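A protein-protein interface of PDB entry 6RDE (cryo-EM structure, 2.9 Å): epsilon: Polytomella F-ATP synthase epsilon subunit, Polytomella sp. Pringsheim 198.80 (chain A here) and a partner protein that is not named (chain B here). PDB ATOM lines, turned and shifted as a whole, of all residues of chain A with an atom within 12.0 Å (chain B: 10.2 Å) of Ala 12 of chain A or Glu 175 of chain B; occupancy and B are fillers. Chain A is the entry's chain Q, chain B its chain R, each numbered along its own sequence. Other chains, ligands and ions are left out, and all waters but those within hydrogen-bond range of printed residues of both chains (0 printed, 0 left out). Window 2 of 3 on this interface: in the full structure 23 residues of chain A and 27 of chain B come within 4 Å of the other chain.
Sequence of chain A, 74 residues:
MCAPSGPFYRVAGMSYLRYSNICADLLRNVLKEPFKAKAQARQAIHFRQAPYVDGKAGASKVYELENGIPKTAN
Among the printed residues, merely in contact across the chains: Phe 8 of chain A with Ala 179 of chain B (3.2 Å), Phe 8 of chain A with Arg 182 of chain B (3.4 Å), Phe 8 of chain A with Ala 183 of chain B (3.7 Å), Ala 12 of chain A with Phe 176 of chain B (3.9 Å), Ala 12 of chain A with Ala 179 of chain B (3.6 Å), Gly 13 of chain A with Phe 176 of chain B (3.3 Å), Met 14 of chain A with Phe 176 of chain B (3.5 Å), Met 14 of chain A with Ala 179 of chain B (3.8 Å), Arg 18 of chain A with Phe 176 of chain B (3.6 Å), Tyr 19 of chain A with Ala 183 of chain B (3.6 Å), Lys 71 of chain A with Phe 176 of chain B (3.2 Å), Thr 72 of chain A with Phe 176 of chain B (3.4 Å) and Ala 73 of chain A with Phe 176 of chain B (3.6 Å).
Ala 12 of chain A touches just these residues of chain B: Glu 175 (3.2 Å), Phe 176 (3.9 Å) and Ala 179 (3.6 Å). Glu 175 of chain B touches one residue of chain A. Of chain B, only Phe 176 comes within 4 Å of Gly 13 of chain A. Asp 174 of chain B touches none of the printed residues of chain A. Phe 176 of chain B touches just these residues of chain A: Ala 12, Gly 13, Met 14, Arg 18, Lys 71, Thr 72 and Ala 73. No residue of chain A comes within 4 Å of Gln 178 of chain B. Ala 179 of chain B touches three residues of chain A. Of the printed residues of chain B, Phe 8 of chain A touches Ala 179 (3.2 Å), Arg 182 (3.4 Å) and Ala 183 (3.7 Å). Of the printed residues of chain A, Arg 182 of chain B touches Phe 8 (3.4 Å). Of the printed residues of chain A, Ala 183 of chain B touches Phe 8 and Tyr 19. Of the printed residues of chain B, Tyr 19 of chain A touches Ala 183 (3.6 Å). Ala 3 of chain A touches none of the printed residues of chain B. Glu 177 of chain B touches none of the printed residues of chain A.
OE1 of Glu 175 of chain B sits close to O of Ala 12 of chain A, 3.2 Å away.
Of the 22 printed residues of chain A, 9 touch a printed residue of chain B. Hydrophobic or aromatic side chains of chain A within 4 Å of the printed part of chain B: Phe 8, Ala 12, Met 14, Tyr 19 and Ala 73. Printed residues of chain B that touch a printed residue of chain A: Glu 175, Phe 176, Ala 179, Arg 182 and Ala 183. Hydrophobic or aromatic side chains of chain B within 4 Å of the printed part of chain A: Phe 176, Ala 179 and Ala 183. Along chain B the printed residues that touch a printed residue of chain A span positions 175 to 183. Among the printed residues, 14 pairs touch across the chains. Among the printed residues, no Asp or Glu carboxylate lies within 4 Å of a Lys or Arg side-chain nitrogen of the other chain.
The backbone carbonyl oxygen of Tyr 9 of chain A sits at hydrogen-bond distance from the backbone NH of Met 14 of chain A (3.0 Å). The side-chain hydroxyl (OG) of Ser 15 of chain A sits at hydrogen-bond distance from the backbone NH (N) of Arg 18 of chain A (3.1 Å). NH1 of Arg 18 of chain A lies close to ND2 of Asn 74 of chain A (3.2 Å).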
ATOM      1  N   ALA A   3     -17.668  -5.246  32.519  1.00  0.00           N
ATOM      2  CA  ALA A   3     -18.787  -4.539  33.138  1.00  0.00           C
ATOM      3  C   ALA A   3     -20.187  -5.189  32.964  1.00  0.00           C
ATOM      4  O   ALA A   3     -20.765  -5.602  33.970  1.00  0.00           O
ATOM      5  CB  ALA A   3     -18.816  -3.077  32.653  1.00  0.00           C
ATOM      6  N   PRO A   4     -20.735  -5.301  31.745  1.00  0.00           N
ATOM      7  CA  PRO A   4     -22.186  -5.472  31.626  1.00  0.00           C
ATOM      8  C   PRO A   4     -22.635  -6.908  31.863  1.00  0.00           C
ATOM      9  O   PRO A   4     -21.836  -7.832  32.022  1.00  0.00           O
ATOM     10  CB  PRO A   4     -22.475  -5.045  30.181  1.00  0.00           C
ATOM     11  CG  PRO A   4     -21.134  -5.077  29.468  1.00  0.00           C
ATOM     12  CD  PRO A   4     -20.113  -5.585  30.434  1.00  0.00           C
ATOM     13  N   SER A   5     -23.951  -7.074  31.905  1.00  0.00           N
ATOM     14  CA  SER A   5     -24.585  -8.375  32.075  1.00  0.00           C
ATOM     15  C   SER A   5     -25.577  -8.583  30.939  1.00  0.00           C
ATOM     16  O   SER A   5     -26.383  -7.692  30.649  1.00  0.00           O
ATOM     17  CB  SER A   5     -25.284  -8.465  33.432  1.00  0.00           C
ATOM     18  OG  SER A   5     -25.950  -9.706  33.598  1.00  0.00           O
ATOM     19  N   GLY A   6     -25.509  -9.741  30.290  1.00  0.00           N
ATOM     20  CA  GLY A   6     -26.463 -10.086  29.266  1.00  0.00           C
ATOM     21  C   GLY A   6     -25.962 -11.179  28.351  1.00  0.00           C
ATOM     22  O   GLY A   6     -25.141 -12.010  28.738  1.00  0.00           O
ATOM     23  N   PRO A   7     -26.450 -11.199  27.113  1.00  0.00           N
ATOM     24  CA  PRO A   7     -25.952 -12.176  26.137  1.00  0.00           C
ATOM     25  C   PRO A   7     -24.559 -11.866  25.624  1.00  0.00           C
ATOM     26  O   PRO A   7     -23.922 -10.909  26.067  1.00  0.00           O
ATOM     27  CB  PRO A   7     -26.985 -12.090  25.012  1.00  0.00           C
ATOM     28  CG  PRO A   7     -28.203 -11.573  25.667  1.00  0.00           C
ATOM     29  CD  PRO A   7     -27.724 -10.611  26.683  1.00  0.00           C
ATOM     30  N   PHE A   8     -24.079 -12.664  24.671  1.00  0.00           N
ATOM     31  CA  PHE A   8     -22.708 -12.519  24.203  1.00  0.00           C
ATOM     32  C   PHE A   8     -22.502 -11.283  23.346  1.00  0.00           C
ATOM     33  O   PHE A   8     -21.372 -10.798  23.247  1.00  0.00           O
ATOM     34  CB  PHE A   8     -22.271 -13.759  23.431  1.00  0.00           C
ATOM     35  CG  PHE A   8     -22.891 -13.893  22.072  1.00  0.00           C
ATOM     36  CD1 PHE A   8     -22.174 -13.571  20.931  1.00  0.00           C
ATOM     37  CD2 PHE A   8     -24.171 -14.389  21.931  1.00  0.00           C
ATOM     38  CE1 PHE A   8     -22.736 -13.706  19.691  1.00  0.00           C
ATOM     39  CE2 PHE A   8     -24.733 -14.528  20.687  1.00  0.00           C
ATOM     40  CZ  PHE A   8     -24.016 -14.187  19.568  1.00  0.00           C
ATOM     41  N   TYR A   9     -23.551 -10.773  22.709  1.00  0.00           N
ATOM     42  CA  TYR A   9     -23.422  -9.487  22.047  1.00  0.00           C
ATOM     43  C   TYR A   9     -23.492  -8.338  23.040  1.00  0.00           C
ATOM     44  O   TYR A   9     -22.829  -7.318  22.845  1.00  0.00           O
ATOM     45  CB  TYR A   9     -24.494  -9.330  20.968  1.00  0.00           C
ATOM     46  CG  TYR A   9     -25.903  -9.684  21.381  1.00  0.00           C
ATOM     47  CD1 TYR A   9     -26.421 -10.942  21.125  1.00  0.00           C
ATOM     48  CD2 TYR A   9     -26.724  -8.749  21.986  1.00  0.00           C
ATOM     49  CE1 TYR A   9     -27.706 -11.264  21.485  1.00  0.00           C
ATOM     50  CE2 TYR A   9     -28.009  -9.064  22.352  1.00  0.00           C
ATOM     51  CZ  TYR A   9     -28.494 -10.321  22.096  1.00  0.00           C
ATOM     52  OH  TYR A   9     -29.776 -10.639  22.453  1.00  0.00           O
ATOM     53  N   ARG A  10     -24.262  -8.496  24.115  1.00  0.00           N
ATOM     54  CA  ARG A  10     -24.458  -7.405  25.061  1.00  0.00           C
ATOM     55  C   ARG A  10     -23.236  -7.202  25.938  1.00  0.00           C
ATOM     56  O   ARG A  10     -22.964  -6.074  26.363  1.00  0.00           O
ATOM     57  CB  ARG A  10     -25.694  -7.678  25.914  1.00  0.00           C
ATOM     58  CG  ARG A  10     -26.164  -6.537  26.790  1.00  0.00           C
ATOM     59  CD  ARG A  10     -26.644  -5.364  25.969  1.00  0.00           C
ATOM     60  NE  ARG A  10     -27.864  -5.658  25.228  1.00  0.00           N
ATOM     61  CZ  ARG A  10     -28.547  -4.751  24.540  1.00  0.00           C
ATOM     62  NH1 ARG A  10     -28.129  -3.498  24.505  1.00  0.00           N
ATOM     63  NH2 ARG A  10     -29.650  -5.090  23.894  1.00  0.00           N
ATOM     64  N   VAL A  11     -22.480  -8.271  26.209  1.00  0.00           N
ATOM     65  CA  VAL A  11     -21.290  -8.154  27.050  1.00  0.00           C
ATOM     66  C   VAL A  11     -20.072  -7.683  26.279  1.00  0.00           C
ATOM     67  O   VAL A  11     -19.029  -7.428  26.891  1.00  0.00           O
ATOM     68  CB  VAL A  11     -20.916  -9.481  27.731  1.00  0.00           C
ATOM     69  CG1 VAL A  11     -21.980  -9.886  28.747  1.00  0.00           C
ATOM     70  CG2 VAL A  11     -20.683 -10.555  26.695  1.00  0.00           C
ATOM     71  N   ALA A  12     -20.170  -7.562  24.957  1.00  0.00           N
ATOM     72  CA  ALA A  12     -19.071  -7.079  24.135  1.00  0.00           C
ATOM     73  C   ALA A  12     -19.267  -5.650  23.656  1.00  0.00           C
ATOM     74  O   ALA A  12     -18.465  -5.167  22.852  1.00  0.00           O
ATOM     75  CB  ALA A  12     -18.867  -7.988  22.935  1.00  0.00           C
ATOM     76  N   GLY A  13     -20.301  -4.960  24.128  1.00  0.00           N
ATOM     77  CA  GLY A  13     -20.548  -3.610  23.671  1.00  0.00           C
ATOM     78  C   GLY A  13     -21.287  -3.506  22.358  1.00  0.00           C
ATOM     79  O   GLY A  13     -21.131  -2.501  21.657  1.00  0.00           O
ATOM     80  N   MET A  14     -22.073  -4.517  21.999  1.00  0.00           N
ATOM     81  CA  MET A  14     -22.853  -4.535  20.770  1.00  0.00           C
ATOM     82  C   MET A  14     -24.335  -4.590  21.118  1.00  0.00           C
ATOM     83  O   MET A  14     -24.743  -5.374  21.977  1.00  0.00           O
ATOM     84  CB  MET A  14     -22.454  -5.733  19.913  1.00  0.00           C
ATOM     85  CG  MET A  14     -23.286  -5.941  18.683  1.00  0.00           C
ATOM     86  SD  MET A  14     -22.934  -7.532  17.943  1.00  0.00           S
ATOM     87  CE  MET A  14     -21.175  -7.391  17.730  1.00  0.00           C
ATOM     88  N   SER A  15     -25.136  -3.759  20.461  1.00  0.00           N
ATOM     89  CA  SER A  15     -26.560  -3.698  20.757  1.00  0.00           C
ATOM     90  C   SER A  15     -27.282  -4.889  20.135  1.00  0.00           C
ATOM     91  O   SER A  15     -26.687  -5.728  19.460  1.00  0.00           O
ATOM     92  CB  SER A  15     -27.148  -2.382  20.260  1.00  0.00           C
ATOM     93  OG  SER A  15     -27.055  -2.286  18.852  1.00  0.00           O
ATOM     94  N   TYR A  16     -28.593  -4.970  20.363  1.00  0.00           N
ATOM     95  CA  TYR A  16     -29.358  -6.019  19.705  1.00  0.00           C
ATOM     96  C   TYR A  16     -29.551  -5.710  18.233  1.00  0.00           C
ATOM     97  O   TYR A  16     -29.518  -6.615  17.392  1.00  0.00           O
ATOM     98  CB  TYR A  16     -30.714  -6.211  20.360  1.00  0.00           C
ATOM     99  CG  TYR A  16     -31.453  -7.332  19.686  1.00  0.00           C
ATOM    100  CD1 TYR A  16     -30.978  -8.629  19.766  1.00  0.00           C
ATOM    101  CD2 TYR A  16     -32.590  -7.096  18.929  1.00  0.00           C
ATOM    102  CE1 TYR A  16     -31.614  -9.660  19.146  1.00  0.00           C
ATOM    103  CE2 TYR A  16     -33.238  -8.135  18.297  1.00  0.00           C
ATOM    104  CZ  TYR A  16     -32.739  -9.415  18.413  1.00  0.00           C
ATOM    105  OH  TYR A  16     -33.364 -10.468  17.799  1.00  0.00           O
ATOM    106  N   ARG A  18     -27.531  -4.019  16.350  1.00  0.00           N
ATOM    107  CA  ARG A  18     -26.299  -4.276  15.631  1.00  0.00           C
ATOM    108  C   ARG A  18     -26.032  -5.762  15.498  1.00  0.00           C
ATOM    109  O   ARG A  18     -25.453  -6.190  14.499  1.00  0.00           O
ATOM    110  CB  ARG A  18     -25.127  -3.595  16.316  1.00  0.00           C
ATOM    111  CG  ARG A  18     -24.046  -3.259  15.347  1.00  0.00           C
ATOM    112  CD  ARG A  18     -23.001  -2.422  16.003  1.00  0.00           C
ATOM    113  NE  ARG A  18     -23.399  -1.032  16.155  1.00  0.00           N
ATOM    114  CZ  ARG A  18     -22.717  -0.022  15.640  1.00  0.00           C
ATOM    115  NH1 ARG A  18     -21.617  -0.262  14.943  1.00  0.00           N
ATOM    116  NH2 ARG A  18     -23.130   1.221  15.826  1.00  0.00           N
ATOM    117  N   TYR A  19     -26.455  -6.556  16.475  1.00  0.00           N
ATOM    118  CA  TYR A  19     -26.256  -7.994  16.387  1.00  0.00           C
ATOM    119  C   TYR A  19     -27.194  -8.612  15.366  1.00  0.00           C
ATOM    120  O   TYR A  19     -26.781  -9.442  14.553  1.00  0.00           O
ATOM    121  CB  TYR A  19     -26.465  -8.639  17.758  1.00  0.00           C
ATOM    122  CG  TYR A  19     -26.824 -10.106  17.702  1.00  0.00           C
ATOM    123  CD1 TYR A  19     -28.129 -10.534  17.939  1.00  0.00           C
ATOM    124  CD2 TYR A  19     -25.860 -11.062  17.424  1.00  0.00           C
ATOM    125  CE1 TYR A  19     -28.461 -11.857  17.882  1.00  0.00           C
ATOM    126  CE2 TYR A  19     -26.184 -12.395  17.375  1.00  0.00           C
ATOM    127  CZ  TYR A  19     -27.486 -12.787  17.604  1.00  0.00           C
ATOM    128  OH  TYR A  19     -27.812 -14.123  17.553  1.00  0.00           O
ATOM    129  N   ILE A  22     -26.408  -7.886  11.736  1.00  0.00           N
ATOM    130  CA  ILE A  22     -25.262  -8.675  11.295  1.00  0.00           C
ATOM    131  C   ILE A  22     -25.713 -10.062  10.852  1.00  0.00           C
ATOM    132  O   ILE A  22     -25.308 -10.553   9.793  1.00  0.00           O
ATOM    133  CB  ILE A  22     -24.209  -8.733  12.418  1.00  0.00           C
ATOM    134  CG1 ILE A  22     -23.325  -7.496  12.375  1.00  0.00           C
ATOM    135  CG2 ILE A  22     -23.338  -9.964  12.316  1.00  0.00           C
ATOM    136  CD1 ILE A  22     -22.442  -7.349  13.585  1.00  0.00           C
ATOM    137  N   PRO A  70     -21.989  -1.532  10.030  1.00  0.00           N
ATOM    138  CA  PRO A  70     -20.586  -1.687  10.439  1.00  0.00           C
ATOM    139  C   PRO A  70     -20.394  -2.833  11.422  1.00  0.00           C
ATOM    140  O   PRO A  70     -20.870  -2.786  12.558  1.00  0.00           O
ATOM    141  CB  PRO A  70     -20.259  -0.340  11.091  1.00  0.00           C
ATOM    142  CG  PRO A  70     -21.145   0.611  10.438  1.00  0.00           C
ATOM    143  CD  PRO A  70     -22.407  -0.121  10.084  1.00  0.00           C
ATOM    144  N   LYS A  71     -19.661  -3.859  10.981  1.00  0.00           N
ATOM    145  CA  LYS A  71     -19.246  -4.935  11.870  1.00  0.00           C
ATOM    146  C   LYS A  71     -18.200  -4.488  12.880  1.00  0.00           C
ATOM    147  O   LYS A  71     -18.015  -5.167  13.895  1.00  0.00           O
ATOM    148  CB  LYS A  71     -18.678  -6.110  11.070  1.00  0.00           C
ATOM    149  CG  LYS A  71     -19.635  -6.787  10.115  1.00  0.00           C
ATOM    150  CD  LYS A  71     -19.072  -8.134   9.677  1.00  0.00           C
ATOM    151  CE  LYS A  71     -20.053  -8.926   8.817  1.00  0.00           C
ATOM    152  NZ  LYS A  71     -20.018  -8.548   7.379  1.00  0.00           N
ATOM    153  N   THR A  72     -17.515  -3.377  12.631  1.00  0.00           N
ATOM    154  CA  THR A  72     -16.430  -2.946  13.493  1.00  0.00           C
ATOM    155  C   THR A  72     -16.963  -2.273  14.750  1.00  0.00           C
ATOM    156  O   THR A  72     -18.124  -1.870  14.836  1.00  0.00           O
ATOM    157  CB  THR A  72     -15.501  -1.988  12.757  1.00  0.00           C
ATOM    158  OG1 THR A  72     -14.488  -1.532  13.659  1.00  0.00           O
ATOM    159  CG2 THR A  72     -16.280  -0.796  12.237  1.00  0.00           C
ATOM    160  N   ALA A  73     -16.083  -2.153  15.736  1.00  0.00           N
ATOM    161  CA  ALA A  73     -16.448  -1.581  17.020  1.00  0.00           C
ATOM    162  C   ALA A  73     -16.588  -0.073  16.898  1.00  0.00           C
ATOM    163  O   ALA A  73     -15.623   0.624  16.567  1.00  0.00           O
ATOM    164  CB  ALA A  73     -15.399  -1.928  18.076  1.00  0.00           C
ATOM    165  N   ASN A  74     -17.785   0.426  17.172  1.00  0.00           N
ATOM    166  CA  ASN A  74     -18.038   1.856  17.112  1.00  0.00           C
ATOM    167  C   ASN A  74     -18.324   2.402  18.505  1.00  0.00           C
ATOM    168  O   ASN A  74     -17.600   2.107  19.457  1.00  0.00           O
ATOM    169  CB  ASN A  74     -19.201   2.155  16.170  1.00  0.00           C
ATOM    170  CG  ASN A  74     -18.836   1.957  14.715  1.00  0.00           C
ATOM    171  OD1 ASN A  74     -17.704   1.608  14.392  1.00  0.00           O
ATOM    172  ND2 ASN A  74     -19.798   2.175  13.827  1.00  0.00           N
ATOM    173  N   GLN B 171      -9.705 -15.710  14.437  1.00  0.00           N
ATOM    174  CA  GLN B 171      -9.737 -15.638  15.894  1.00  0.00           C
ATOM    175  C   GLN B 171      -9.050 -14.340  16.302  1.00  0.00           C
ATOM    176  O   GLN B 171      -7.831 -14.318  16.531  1.00  0.00           O
ATOM    177  CB  GLN B 171      -9.051 -16.850  16.528  1.00  0.00           C
ATOM    178  CG  GLN B 171      -9.714 -18.178  16.177  1.00  0.00           C
ATOM    179  CD  GLN B 171     -11.178 -18.252  16.598  1.00  0.00           C
ATOM    180  OE1 GLN B 171     -12.078 -18.267  15.758  1.00  0.00           O
ATOM    181  NE2 GLN B 171     -11.418 -18.298  17.905  1.00  0.00           N
ATOM    182  N   PRO B 172      -9.781 -13.231  16.390  1.00  0.00           N
ATOM    183  CA  PRO B 172      -9.139 -11.927  16.574  1.00  0.00           C
ATOM    184  C   PRO B 172      -8.991 -11.553  18.036  1.00  0.00           C
ATOM    185  O   PRO B 172      -9.338 -12.335  18.925  1.00  0.00           O
ATOM    186  CB  PRO B 172     -10.089 -10.967  15.847  1.00  0.00           C
ATOM    187  CG  PRO B 172     -11.320 -11.806  15.490  1.00  0.00           C
ATOM    188  CD  PRO B 172     -11.231 -13.087  16.226  1.00  0.00           C
ATOM    189  N   THR B 173      -8.486 -10.347  18.290  1.00  0.00           N
ATOM    190  CA  THR B 173      -8.178  -9.910  19.643  1.00  0.00           C
ATOM    191  C   THR B 173      -9.213  -8.959  20.227  1.00  0.00           C
ATOM    192  O   THR B 173      -9.143  -8.661  21.425  1.00  0.00           O
ATOM    193  CB  THR B 173      -6.805  -9.225  19.680  1.00  0.00           C
ATOM    194  OG1 THR B 173      -6.936  -7.863  19.253  1.00  0.00           O
ATOM    195  CG2 THR B 173      -5.830  -9.934  18.761  1.00  0.00           C
ATOM    196  N   ASP B 174     -10.150  -8.469  19.422  1.00  0.00           N
ATOM    197  CA  ASP B 174     -11.170  -7.564  19.936  1.00  0.00           C
ATOM    198  C   ASP B 174     -12.437  -8.324  20.318  1.00  0.00           C
ATOM    199  O   ASP B 174     -12.789  -9.341  19.713  1.00  0.00           O
ATOM    200  CB  ASP B 174     -11.491  -6.481  18.905  1.00  0.00           C
ATOM    201  CG  ASP B 174     -12.073  -7.047  17.628  1.00  0.00           C
ATOM    202  OD1 ASP B 174     -11.667  -8.164  17.240  1.00  0.00           O
ATOM    203  OD2 ASP B 174     -12.925  -6.371  17.012  1.00  0.00           O
ATOM    204  N   GLU B 175     -13.124  -7.819  21.344  1.00  0.00           N
ATOM    205  CA  GLU B 175     -14.357  -8.441  21.806  1.00  0.00           C
ATOM    206  C   GLU B 175     -15.504  -8.273  20.824  1.00  0.00           C
ATOM    207  O   GLU B 175     -16.392  -9.131  20.780  1.00  0.00           O
ATOM    208  CB  GLU B 175     -14.765  -7.861  23.162  1.00  0.00           C
ATOM    209  CG  GLU B 175     -14.627  -6.347  23.260  1.00  0.00           C
ATOM    210  CD  GLU B 175     -14.913  -5.823  24.657  1.00  0.00           C
ATOM    211  OE1 GLU B 175     -16.041  -5.345  24.902  1.00  0.00           O
ATOM    212  OE2 GLU B 175     -14.009  -5.893  25.516  1.00  0.00           O
ATOM    213  N   PHE B 176     -15.496  -7.199  20.034  1.00  0.00           N
ATOM    214  CA  PHE B 176     -16.602  -6.888  19.137  1.00  0.00           C
ATOM    215  C   PHE B 176     -16.692  -7.893  18.001  1.00  0.00           C
ATOM    216  O   PHE B 176     -17.774  -8.401  17.695  1.00  0.00           O
ATOM    217  CB  PHE B 176     -16.423  -5.480  18.586  1.00  0.00           C
ATOM    218  CG  PHE B 176     -17.706  -4.768  18.294  1.00  0.00           C
ATOM    219  CD1 PHE B 176     -18.240  -3.880  19.212  1.00  0.00           C
ATOM    220  CD2 PHE B 176     -18.361  -4.960  17.090  1.00  0.00           C
ATOM    221  CE1 PHE B 176     -19.405  -3.203  18.941  1.00  0.00           C
ATOM    222  CE2 PHE B 176     -19.532  -4.291  16.816  1.00  0.00           C
ATOM    223  CZ  PHE B 176     -20.052  -3.411  17.746  1.00  0.00           C
ATOM    224  N   GLU B 177     -15.563  -8.192  17.366  1.00  0.00           N
ATOM    225  CA  GLU B 177     -15.562  -9.213  16.328  1.00  0.00           C
ATOM    226  C   GLU B 177     -15.670 -10.609  16.932  1.00  0.00           C
ATOM    227  O   GLU B 177     -16.182 -11.521  16.279  1.00  0.00           O
ATOM    228  CB  GLU B 177     -14.315  -9.051  15.454  1.00  0.00           C
ATOM    229  CG  GLU B 177     -14.189  -9.992  14.263  1.00  0.00           C
ATOM    230  CD  GLU B 177     -15.403 -10.017  13.373  1.00  0.00           C
ATOM    231  OE1 GLU B 177     -15.623  -9.035  12.638  1.00  0.00           O
ATOM    232  OE2 GLU B 177     -16.130 -11.032  13.396  1.00  0.00           O
ATOM    233  N   GLN B 178     -15.240 -10.790  18.183  1.00  0.00           N
ATOM    234  CA  GLN B 178     -15.491 -12.059  18.863  1.00  0.00           C
ATOM    235  C   GLN B 178     -16.982 -12.253  19.134  1.00  0.00           C
ATOM    236  O   GLN B 178     -17.487 -13.380  19.085  1.00  0.00           O
ATOM    237  CB  GLN B 178     -14.683 -12.130  20.159  1.00  0.00           C
ATOM    238  CG  GLN B 178     -14.694 -13.496  20.851  1.00  0.00           C
ATOM    239  CD  GLN B 178     -14.710 -14.657  19.873  1.00  0.00           C
ATOM    240  OE1 GLN B 178     -13.745 -14.887  19.149  1.00  0.00           O
ATOM    241  NE2 GLN B 178     -15.814 -15.394  19.846  1.00  0.00           N
ATOM    242  N   ALA B 179     -17.708 -11.164  19.405  1.00  0.00           N
ATOM    243  CA  ALA B 179     -19.164 -11.241  19.394  1.00  0.00           C
ATOM    244  C   ALA B 179     -19.705 -11.384  17.980  1.00  0.00           C
ATOM    245  O   ALA B 179     -20.801 -11.917  17.789  1.00  0.00           O
ATOM    246  CB  ALA B 179     -19.770 -10.009  20.048  1.00  0.00           C
ATOM    247  N   ALA B 180     -18.966 -10.897  16.983  1.00  0.00           N
ATOM    248  CA  ALA B 180     -19.445 -10.953  15.610  1.00  0.00           C
ATOM    249  C   ALA B 180     -19.059 -12.253  14.935  1.00  0.00           C
ATOM    250  O   ALA B 180     -19.788 -12.724  14.059  1.00  0.00           O
ATOM    251  CB  ALA B 180     -18.916  -9.766  14.808  1.00  0.00           C
ATOM    252  N   ASN B 181     -17.924 -12.845  15.316  1.00  0.00           N
ATOM    253  CA  ASN B 181     -17.568 -14.149  14.772  1.00  0.00           C
ATOM    254  C   ASN B 181     -18.407 -15.259  15.380  1.00  0.00           C
ATOM    255  O   ASN B 181     -18.783 -16.190  14.665  1.00  0.00           O
ATOM    256  CB  ASN B 181     -16.089 -14.454  14.996  1.00  0.00           C
ATOM    257  CG  ASN B 181     -15.530 -15.389  13.956  1.00  0.00           C
ATOM    258  OD1 ASN B 181     -15.997 -15.419  12.819  1.00  0.00           O
ATOM    259  ND2 ASN B 181     -14.519 -16.158  14.337  1.00  0.00           N
ATOM    260  N   ARG B 182     -18.713 -15.172  16.679  1.00  0.00           N
ATOM    261  CA  ARG B 182     -19.582 -16.163  17.304  1.00  0.00           C
ATOM    262  C   ARG B 182     -20.977 -16.112  16.708  1.00  0.00           C
ATOM    263  O   ARG B 182     -21.586 -17.157  16.451  1.00  0.00           O
ATOM    264  CB  ARG B 182     -19.641 -15.944  18.810  1.00  0.00           C
ATOM    265  CG  ARG B 182     -20.509 -16.960  19.505  1.00  0.00           C
ATOM    266  CD  ARG B 182     -20.486 -16.817  21.000  1.00  0.00           C
ATOM    267  NE  ARG B 182     -21.754 -17.254  21.558  1.00  0.00           N
ATOM    268  CZ  ARG B 182     -22.024 -17.284  22.852  1.00  0.00           C
ATOM    269  NH1 ARG B 182     -21.103 -16.906  23.727  1.00  0.00           N
ATOM    270  NH2 ARG B 182     -23.213 -17.692  23.267  1.00  0.00           N
ATOM    271  N   ALA B 183     -21.467 -14.906  16.425  1.00  0.00           N
ATOM    272  CA  ALA B 183     -22.686 -14.743  15.648  1.00  0.00           C
ATOM    273  C   ALA B 183     -22.516 -15.180  14.200  1.00  0.00           C
ATOM    274  O   ALA B 183     -23.510 -15.519  13.551  1.00  0.00           O
ATOM    275  CB  ALA B 183     -23.135 -13.286  15.692  1.00  0.00           C
